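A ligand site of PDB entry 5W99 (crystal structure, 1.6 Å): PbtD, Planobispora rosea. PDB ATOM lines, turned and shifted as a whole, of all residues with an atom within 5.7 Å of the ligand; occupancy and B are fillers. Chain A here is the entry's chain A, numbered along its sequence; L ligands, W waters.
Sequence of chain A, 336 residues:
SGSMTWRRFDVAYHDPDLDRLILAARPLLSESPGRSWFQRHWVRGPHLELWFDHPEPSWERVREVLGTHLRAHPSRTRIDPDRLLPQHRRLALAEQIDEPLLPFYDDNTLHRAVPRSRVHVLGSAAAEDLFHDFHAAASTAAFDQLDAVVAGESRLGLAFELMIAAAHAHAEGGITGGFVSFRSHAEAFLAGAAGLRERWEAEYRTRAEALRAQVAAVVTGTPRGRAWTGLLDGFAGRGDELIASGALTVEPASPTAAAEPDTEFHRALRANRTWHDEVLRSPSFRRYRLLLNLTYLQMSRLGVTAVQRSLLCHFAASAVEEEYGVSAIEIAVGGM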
ATOM      1  N   GLU A 172     -13.987  -1.614 -32.657  1.00  0.00           N
ATOM      2  CA  GLU A 172     -12.672  -1.305 -32.148  1.00  0.00           C
ATOM      3  C   GLU A 172     -12.736  -1.203 -30.590  1.00  0.00           C
ATOM      4  O   GLU A 172     -13.673  -0.607 -29.983  1.00  0.00           O
ATOM      5  CB  GLU A 172     -12.064  -0.065 -32.823  1.00  0.00           C
ATOM      6  CG  GLU A 172     -10.956  -0.515 -33.782  1.00  0.00           C
ATOM      7  CD  GLU A 172      -9.783   0.392 -33.663  1.00  0.00           C
ATOM      8  OE1 GLU A 172      -9.882   1.505 -34.187  1.00  0.00           O
ATOM      9  OE2 GLU A 172      -8.801   0.021 -33.005  1.00  0.00           O
ATOM     10  N   GLY A 173     -11.810  -1.896 -29.986  1.00  0.00           N
ATOM     11  CA  GLY A 173     -11.722  -1.936 -28.553  1.00  0.00           C
ATOM     12  C   GLY A 173     -12.592  -3.048 -27.990  1.00  0.00           C
ATOM     13  O   GLY A 173     -12.561  -3.272 -26.771  1.00  0.00           O
ATOM     14  N   THR A 176     -15.904  -3.384 -24.588  1.00  0.00           N
ATOM     15  CA  THR A 176     -15.834  -2.137 -23.818  1.00  0.00           C
ATOM     16  C   THR A 176     -15.654  -0.907 -24.657  1.00  0.00           C
ATOM     17  O   THR A 176     -15.606   0.181 -24.097  1.00  0.00           O
ATOM     18  CB  THR A 176     -14.784  -2.182 -22.679  1.00  0.00           C
ATOM     19  OG1 THR A 176     -13.506  -2.345 -23.255  1.00  0.00           O
ATOM     20  CG2 THR A 176     -15.046  -3.265 -21.694  1.00  0.00           C
ATOM     21  N   GLY A 177     -15.571  -1.084 -25.981  1.00  0.00           N
ATOM     22  CA  GLY A 177     -15.736   0.004 -26.959  1.00  0.00           C
ATOM     23  C   GLY A 177     -17.113  -0.006 -27.544  1.00  0.00           C
ATOM     24  O   GLY A 177     -17.867   1.003 -27.523  1.00  0.00           O
ATOM     25  N   GLY A 178     -17.488  -1.143 -28.140  1.00  0.00           N
ATOM     26  CA  GLY A 178     -18.741  -1.201 -28.908  1.00  0.00           C
ATOM     27  C   GLY A 178     -20.015  -0.971 -28.110  1.00  0.00           C
ATOM     28  O   GLY A 178     -21.015  -0.495 -28.646  1.00  0.00           O
ATOM     29  N   VAL A 180     -20.759   1.380 -26.122  1.00  0.00           N
ATOM     30  CA  VAL A 180     -21.186   2.782 -26.037  1.00  0.00           C
ATOM     31  C   VAL A 180     -22.298   3.030 -27.077  1.00  0.00           C
ATOM     32  O   VAL A 180     -23.272   3.770 -26.832  1.00  0.00           O
ATOM     33  CB  VAL A 180     -19.981   3.733 -26.276  1.00  0.00           C
ATOM     34  CG1 VAL A 180     -20.414   5.184 -26.268  1.00  0.00           C
ATOM     35  CG2 VAL A 180     -18.888   3.479 -25.237  1.00  0.00           C
ATOM     36  N   SER A 181     -22.230   2.330 -28.208  1.00  0.00           N
ATOM     37  CA  SER A 181     -23.284   2.418 -29.204  1.00  0.00           C
ATOM     38  C   SER A 181     -24.660   1.971 -28.649  1.00  0.00           C
ATOM     39  O   SER A 181     -25.712   2.507 -29.004  1.00  0.00           O
ATOM     40  CB  SER A 181     -22.968   1.630 -30.521  1.00  0.00           C
ATOM     41  OG  SER A 181     -21.800   2.169 -31.120  1.00  0.00           O
ATOM     42  N   SER A 184     -26.089   4.706 -26.619  1.00  0.00           N
ATOM     43  CA  SER A 184     -26.502   5.730 -27.534  1.00  0.00           C
ATOM     44  C   SER A 184     -27.861   5.417 -28.125  1.00  0.00           C
ATOM     45  O   SER A 184     -28.780   6.244 -28.158  1.00  0.00           O
ATOM     46  CB  SER A 184     -25.474   5.888 -28.686  1.00  0.00           C
ATOM     47  OG  SER A 184     -25.975   6.845 -29.596  1.00  0.00           O
ATOM     48  N   HIS A 185     -28.041   4.193 -28.556  1.00  0.00           N
ATOM     49  CA  HIS A 185     -29.286   3.822 -29.210  1.00  0.00           C
ATOM     50  C   HIS A 185     -30.462   3.779 -28.246  1.00  0.00           C
ATOM     51  O   HIS A 185     -31.581   4.253 -28.594  1.00  0.00           O
ATOM     52  CB  HIS A 185     -29.181   2.511 -30.016  1.00  0.00           C
ATOM     53  CG  HIS A 185     -28.054   2.520 -31.020  1.00  0.00           C
ATOM     54  ND1 HIS A 185     -27.554   1.378 -31.640  1.00  0.00           N
ATOM     55  CD2 HIS A 185     -27.268   3.543 -31.429  1.00  0.00           C
ATOM     56  CE1 HIS A 185     -26.514   1.707 -32.383  1.00  0.00           C
ATOM     57  NE2 HIS A 185     -26.347   3.023 -32.312  1.00  0.00           N
ATOM     58  N   PHE A 265     -26.713  12.296 -22.766  1.00  0.00           N
ATOM     59  CA  PHE A 265     -25.662  11.525 -23.438  1.00  0.00           C
ATOM     60  C   PHE A 265     -25.231  12.155 -24.744  1.00  0.00           C
ATOM     61  O   PHE A 265     -24.020  12.223 -25.022  1.00  0.00           O
ATOM     62  CB  PHE A 265     -26.162  10.071 -23.674  1.00  0.00           C
ATOM     63  CG  PHE A 265     -25.186   9.192 -24.355  1.00  0.00           C
ATOM     64  CD1 PHE A 265     -24.266   8.447 -23.646  1.00  0.00           C
ATOM     65  CD2 PHE A 265     -25.214   9.103 -25.729  1.00  0.00           C
ATOM     66  CE1 PHE A 265     -23.332   7.682 -24.307  1.00  0.00           C
ATOM     67  CE2 PHE A 265     -24.286   8.285 -26.398  1.00  0.00           C
ATOM     68  CZ  PHE A 265     -23.337   7.584 -25.679  1.00  0.00           C
ATOM     69  N   HIS A 266     -26.184  12.555 -25.576  1.00  0.00           N
ATOM     70  CA  HIS A 266     -25.809  13.009 -26.904  1.00  0.00           C
ATOM     71  C   HIS A 266     -25.239  14.460 -26.854  1.00  0.00           C
ATOM     72  O   HIS A 266     -24.368  14.782 -27.660  1.00  0.00           O
ATOM     73  CB  HIS A 266     -26.889  12.806 -27.916  1.00  0.00           C
ATOM     74  CG  HIS A 266     -27.229  11.364 -28.124  1.00  0.00           C
ATOM     75  ND1 HIS A 266     -28.238  10.699 -27.436  1.00  0.00           N
ATOM     76  CD2 HIS A 266     -26.624  10.433 -28.909  1.00  0.00           C
ATOM     77  CE1 HIS A 266     -28.286   9.444 -27.864  1.00  0.00           C
ATOM     78  NE2 HIS A 266     -27.292   9.235 -28.721  1.00  0.00           N
ATOM     79  N   LEU A 269     -21.663  13.877 -26.036  1.00  0.00           N
ATOM     80  CA  LEU A 269     -20.944  13.333 -27.137  1.00  0.00           C
ATOM     81  C   LEU A 269     -20.600  14.423 -28.128  1.00  0.00           C
ATOM     82  O   LEU A 269     -19.466  14.507 -28.633  1.00  0.00           O
ATOM     83  CB  LEU A 269     -21.838  12.243 -27.754  1.00  0.00           C
ATOM     84  CG  LEU A 269     -21.306  11.299 -28.722  1.00  0.00           C
ATOM     85  CD1 LEU A 269     -20.235  10.396 -28.082  1.00  0.00           C
ATOM     86  CD2 LEU A 269     -22.460  10.463 -29.256  1.00  0.00           C
ATOM     87  N   ASN A 272     -17.422  16.301 -27.399  1.00  0.00           N
ATOM     88  CA  ASN A 272     -16.242  15.470 -27.146  1.00  0.00           C
ATOM     89  C   ASN A 272     -15.499  15.422 -28.454  1.00  0.00           C
ATOM     90  O   ASN A 272     -15.976  14.806 -29.423  1.00  0.00           O
ATOM     91  CB  ASN A 272     -16.726  14.094 -26.641  1.00  0.00           C
ATOM     92  CG  ASN A 272     -15.571  13.125 -26.393  1.00  0.00           C
ATOM     93  OD1 ASN A 272     -14.534  13.191 -27.041  1.00  0.00           O
ATOM     94  ND2 ASN A 272     -15.803  12.115 -25.497  1.00  0.00           N
ATOM     95  N   THR A 274     -12.911  13.737 -29.355  1.00  0.00           N
ATOM     96  CA  THR A 274     -12.530  12.382 -29.756  1.00  0.00           C
ATOM     97  C   THR A 274     -13.643  11.709 -30.532  1.00  0.00           C
ATOM     98  O   THR A 274     -13.405  10.981 -31.506  1.00  0.00           O
ATOM     99  CB  THR A 274     -12.141  11.542 -28.526  1.00  0.00           C
ATOM    100  OG1 THR A 274     -10.977  12.147 -27.896  1.00  0.00           O
ATOM    101  CG2 THR A 274     -11.830  10.095 -28.921  1.00  0.00           C
ATOM    102  N   TRP A 275     -14.847  12.001 -30.110  1.00  0.00           N
ATOM    103  CA  TRP A 275     -16.023  11.502 -30.916  1.00  0.00           C
ATOM    104  C   TRP A 275     -15.936  11.983 -32.353  1.00  0.00           C
ATOM    105  O   TRP A 275     -16.021  11.214 -33.314  1.00  0.00           O
ATOM    106  CB  TRP A 275     -17.365  11.883 -30.270  1.00  0.00           C
ATOM    107  CG  TRP A 275     -18.546  11.879 -31.194  1.00  0.00           C
ATOM    108  CD1 TRP A 275     -19.222  12.952 -31.647  1.00  0.00           C
ATOM    109  CD2 TRP A 275     -19.212  10.732 -31.750  1.00  0.00           C
ATOM    110  NE1 TRP A 275     -20.292  12.553 -32.428  1.00  0.00           N
ATOM    111  CE2 TRP A 275     -20.295  11.208 -32.513  1.00  0.00           C
ATOM    112  CE3 TRP A 275     -18.989   9.373 -31.660  1.00  0.00           C
ATOM    113  CZ2 TRP A 275     -21.189  10.344 -33.204  1.00  0.00           C
ATOM    114  CZ3 TRP A 275     -19.870   8.505 -32.371  1.00  0.00           C
ATOM    115  CH2 TRP A 275     -20.909   9.021 -33.158  1.00  0.00           C
ATOM    116  N   VAL A 279     -13.774   8.696 -33.665  1.00  0.00           N
ATOM    117  CA  VAL A 279     -14.863   7.702 -33.658  1.00  0.00           C
ATOM    118  C   VAL A 279     -15.719   7.841 -34.920  1.00  0.00           C
ATOM    119  O   VAL A 279     -15.632   7.008 -35.874  1.00  0.00           O
ATOM    120  CB  VAL A 279     -15.710   7.708 -32.346  1.00  0.00           C
ATOM    121  CG1 VAL A 279     -16.744   6.560 -32.387  1.00  0.00           C
ATOM    122  CG2 VAL A 279     -14.832   7.538 -31.118  1.00  0.00           C
ATOM    123  N   PHE A 285     -15.205   2.454 -37.169  1.00  0.00           N
ATOM    124  CA  PHE A 285     -16.568   2.683 -36.527  1.00  0.00           C
ATOM    125  C   PHE A 285     -17.650   2.545 -37.588  1.00  0.00           C
ATOM    126  O   PHE A 285     -18.739   2.011 -37.308  1.00  0.00           O
ATOM    127  CB  PHE A 285     -16.609   4.047 -35.892  1.00  0.00           C
ATOM    128  CG  PHE A 285     -17.953   4.420 -35.310  1.00  0.00           C
ATOM    129  CD1 PHE A 285     -18.430   3.821 -34.149  1.00  0.00           C
ATOM    130  CD2 PHE A 285     -18.750   5.380 -35.925  1.00  0.00           C
ATOM    131  CE1 PHE A 285     -19.685   4.195 -33.638  1.00  0.00           C
ATOM    132  CE2 PHE A 285     -19.960   5.780 -35.409  1.00  0.00           C
ATOM    133  CZ  PHE A 285     -20.412   5.166 -34.254  1.00  0.00           C
ATOM    134  N   TYR A 288     -18.183  -1.170 -38.030  1.00  0.00           N
ATOM    135  CA  TYR A 288     -18.930  -1.656 -36.855  1.00  0.00           C
ATOM    136  C   TYR A 288     -20.405  -1.290 -36.980  1.00  0.00           C
ATOM    137  O   TYR A 288     -21.290  -2.150 -36.746  1.00  0.00           O
ATOM    138  CB  TYR A 288     -18.327  -1.117 -35.557  1.00  0.00           C
ATOM    139  CG  TYR A 288     -19.158  -1.420 -34.328  1.00  0.00           C
ATOM    140  CD1 TYR A 288     -19.604  -2.669 -34.044  1.00  0.00           C
ATOM    141  CD2 TYR A 288     -19.503  -0.406 -33.449  1.00  0.00           C
ATOM    142  CE1 TYR A 288     -20.400  -2.920 -32.896  1.00  0.00           C
ATOM    143  CE2 TYR A 288     -20.210  -0.640 -32.300  1.00  0.00           C
ATOM    144  CZ  TYR A 288     -20.683  -1.897 -32.033  1.00  0.00           C
ATOM    145  OH  TYR A 288     -21.455  -2.163 -30.876  1.00  0.00           O
ATOM    146  N   ARG A 289     -20.690  -0.020 -37.275  1.00  0.00           N
ATOM    147  CA  ARG A 289     -22.067   0.424 -37.326  1.00  0.00           C
ATOM    148  C   ARG A 289     -22.864  -0.276 -38.424  1.00  0.00           C
ATOM    149  O   ARG A 289     -24.042  -0.606 -38.212  1.00  0.00           O
ATOM    150  CB  ARG A 289     -22.158   1.898 -37.381  1.00  0.00           C
ATOM    151  CG  ARG A 289     -21.877   2.566 -36.002  1.00  0.00           C
ATOM    152  CD  ARG A 289     -22.964   2.349 -34.942  1.00  0.00           C
ATOM    153  NE  ARG A 289     -24.210   3.053 -35.253  1.00  0.00           N
ATOM    154  CZ  ARG A 289     -25.352   2.534 -35.688  1.00  0.00           C
ATOM    155  NH1 ARG A 289     -25.461   1.182 -35.960  1.00  0.00           N
ATOM    156  NH2 ARG A 289     -26.440   3.360 -35.806  1.00  0.00           N
ATOM    157  N   ILE A 331     -17.632   7.900 -20.729  1.00  0.00           N
ATOM    158  CA  ILE A 331     -16.814   7.850 -21.938  1.00  0.00           C
ATOM    159  C   ILE A 331     -17.286   9.004 -22.813  1.00  0.00           C
ATOM    160  O   ILE A 331     -16.473   9.742 -23.382  1.00  0.00           O
ATOM    161  CB  ILE A 331     -16.912   6.456 -22.665  1.00  0.00           C
ATOM    162  CG1 ILE A 331     -16.102   5.427 -21.879  1.00  0.00           C
ATOM    163  CG2 ILE A 331     -16.387   6.570 -24.101  1.00  0.00           C
ATOM    164  CD1 ILE A 331     -16.508   3.975 -22.242  1.00  0.00           C
ATOM    165  N   ALA A 332     -18.585   9.146 -22.978  1.00  0.00           N
ATOM    166  CA  ALA A 332     -19.110  10.228 -23.859  1.00  0.00           C
ATOM    167  C   ALA A 332     -18.658  11.590 -23.394  1.00  0.00           C
ATOM    168  O   ALA A 332     -18.397  12.468 -24.227  1.00  0.00           O
ATOM    169  CB  ALA A 332     -20.622  10.190 -24.009  1.00  0.00           C
ATOM    170  N   VAL A 333     -18.699  11.815 -22.101  1.00  0.00           N
ATOM    171  CA  VAL A 333     -18.322  13.156 -21.544  1.00  0.00           C
ATOM    172  C   VAL A 333     -16.848  13.447 -21.817  1.00  0.00           C
ATOM    173  O   VAL A 333     -16.487  14.557 -22.253  1.00  0.00           O
ATOM    174  CB  VAL A 333     -18.627  13.239 -20.021  1.00  0.00           C
ATOM    175  CG1 VAL A 333     -18.125  14.556 -19.411  1.00  0.00           C
ATOM    176  CG2 VAL A 333     -20.106  13.167 -19.758  1.00  0.00           C
ATOM    177  N   GLY A 334     -15.992  12.451 -21.630  1.00  0.00           N
ATOM    178  CA  GLY A 334     -14.575  12.587 -21.975  1.00  0.00           C
ATOM    179  C   GLY A 334     -13.733  13.335 -20.951  1.00  0.00           C
ATOM    180  O   GLY A 334     -14.220  13.538 -19.817  1.00  0.00           O
HETATM  181  C1  LIG L   1     -16.835   6.864 -28.016  1.00  0.00           C
HETATM  182  C2  LIG L   1     -17.498   5.725 -28.635  1.00  0.00           C
HETATM  183  C3  LIG L   1     -19.480   5.124 -29.761  1.00  0.00           C
HETATM  184  C4  LIG L   1     -17.799   3.496 -29.517  1.00  0.00           C
HETATM  185  C5  LIG L   1     -13.638   3.008 -28.108  1.00  0.00           C
HETATM  186  C6  LIG L   1     -13.815   3.161 -26.821  1.00  0.00           C
HETATM  187  C7  LIG L   1     -12.334   2.318 -28.715  1.00  0.00           C
HETATM  188  N1  LIG L   1     -12.067  11.334 -23.470  1.00  0.00           N
HETATM  189  C8  LIG L   1     -11.572  10.761 -24.647  1.00  0.00           C
HETATM  190  C9  LIG L   1     -12.424   9.608 -25.304  1.00  0.00           C
HETATM  191  N2  LIG L   1     -13.651   9.644 -25.841  1.00  0.00           N
HETATM  192  C10 LIG L   1     -14.022   8.407 -26.424  1.00  0.00           C
HETATM  193  C11 LIG L   1     -13.083   7.454 -26.236  1.00  0.00           C
HETATM  194  S1  LIG L   1     -11.709   8.100 -25.403  1.00  0.00           S
HETATM  195  C12 LIG L   1     -15.236   8.110 -27.051  1.00  0.00           C
HETATM  196  N3  LIG L   1     -15.545   6.859 -27.587  1.00  0.00           N
HETATM  197  C13 LIG L   1     -17.491   8.052 -27.876  1.00  0.00           C
HETATM  198  S2  LIG L   1     -16.452   9.260 -27.152  1.00  0.00           S
HETATM  199  N4  LIG L   1     -18.717   6.019 -29.088  1.00  0.00           N
HETATM  200  C14 LIG L   1     -19.038   3.843 -30.027  1.00  0.00           C
HETATM  201  C15 LIG L   1     -16.927   4.441 -28.827  1.00  0.00           C
HETATM  202  C16 LIG L   1     -15.622   3.958 -28.307  1.00  0.00           C
HETATM  203  N5  LIG L   1     -14.663   3.455 -28.967  1.00  0.00           N
HETATM  204  S3  LIG L   1     -15.369   3.902 -26.590  1.00  0.00           S
HETATM  205  O1  LIG L   1     -11.536   1.855 -27.932  1.00  0.00           O
HETATM  206  O2  LIG L   1     -12.304   2.266 -29.920  1.00  0.00           O
HETATM  207  C17 LIG L   1     -20.748   5.544 -30.151  1.00  0.00           C
HETATM  208  N6  LIG L   1     -21.670   4.966 -30.908  1.00  0.00           N
HETATM  209  C18 LIG L   1     -22.780   5.793 -31.120  1.00  0.00           C
HETATM  210  C19 LIG L   1     -22.722   6.971 -30.473  1.00  0.00           C
HETATM  211  S4  LIG L   1     -21.302   7.162 -29.518  1.00  0.00           S
HETATM  212  C20 LIG L   1     -23.924   5.346 -31.980  1.00  0.00           C
HETATM  213  O3  LIG L   1     -24.985   6.041 -32.006  1.00  0.00           O
HETATM  214  O4  LIG L   1     -23.805   4.273 -32.595  1.00  0.00           O
HETATM  215  O   HOH W   1     -11.592   0.624 -25.131  1.00  0.00           O
HETATM  216  O   HOH W   2     -12.819   4.537 -23.812  1.00  0.00           O
HETATM  217  O   HOH W   3     -13.764   9.130 -22.192  1.00  0.00           O
HETATM  218  O   HOH W   4     -15.468   0.932 -30.551  1.00  0.00           O
HETATM  219  O   HOH W   5     -26.017   5.833 -34.334  1.00  0.00           O
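The side-chain hydroxyl (OG) of Ser 181 lies within hydrogen-bond range of a nitrogen (N6) of the ligand (2.8 Å). OG of Ser 184 sits at hydrogen-bond distance from O3 of the ligand (2.7 Å). An oxygen (O4) of the ligand is in salt-bridge range of the guanidinium group (NE) of Arg 289, 3.0 Å away. A nitrogen (N2) of the ligand sits at hydrogen-bond distance from the side-chain amide nitrogen (ND2) of Asn 272. NE2 of His 185 sits at hydrogen-bond distance from O4 of the ligand, 2.8 Å away.
The backbone NH (N) of Trp 275 lies within hydrogen-bond range of the side-chain amide oxygen (OD1) of Asn 272 (3.3 Å). O of Ala 332 is in hydrogen-bond range of ND2 of Asn 272 (2.9 Å). OG of Ser 184 is in hydrogen-bond range of NE2 of His 266 (2.9 Å). The backbone carbonyl oxygen (O) of Ser 181 sits close to a ring nitrogen (NE2) of His 185. The side-chain amide nitrogen (ND2) of Asn 272 is in hydrogen-bond range of the backbone carbonyl oxygen (O) of Ile 331 (3.2 Å). The side-chain amide oxygen (OD1) of Asn 272 sits at hydrogen-bond distance from the backbone NH (N) of Thr 274 (2.9 Å). O of Thr 274 lies within hydrogen-bond range of N of Val 279, at 3.2 Å.
O2 of the ligand lies close to O of Glu 172, 3.2 Å away. Residues that only touch the ligand: Gly 334 (3.2 Å), Gly 177 (3.2 Å), Val 180 (3.4 Å), Phe 285 (3.5 Å), Trp 275 (3.5 Å), Leu 269 (3.5 Å), Ile 331 (3.5 Å), Thr 274 (3.6 Å), Val 279 (3.7 Å) and Gly 173 (3.8 Å). Hydrophobic or aromatic side chains that line the ligand: Val 180, His 185, Leu 269, Trp 275, Val 279, Phe 285 and Ile 331. The nearest printed residue that does not touch the ligand is Ala 332 (4.3 Å).
Water W5 lies within hydrogen-bond range of O3 of the ligand, NH2 of Arg 289 and NE2 of His 185. Water W3 lies within hydrogen-bond range of O of Ile 331 (3.0 Å) and N1 of the ligand (3.1 Å). Water W4 lies within hydrogen-bond range of the backbone carbonyl oxygen (O) of Glu 172 (2.4 Å) and a nitrogen (N5) of the ligand (3.1 Å).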
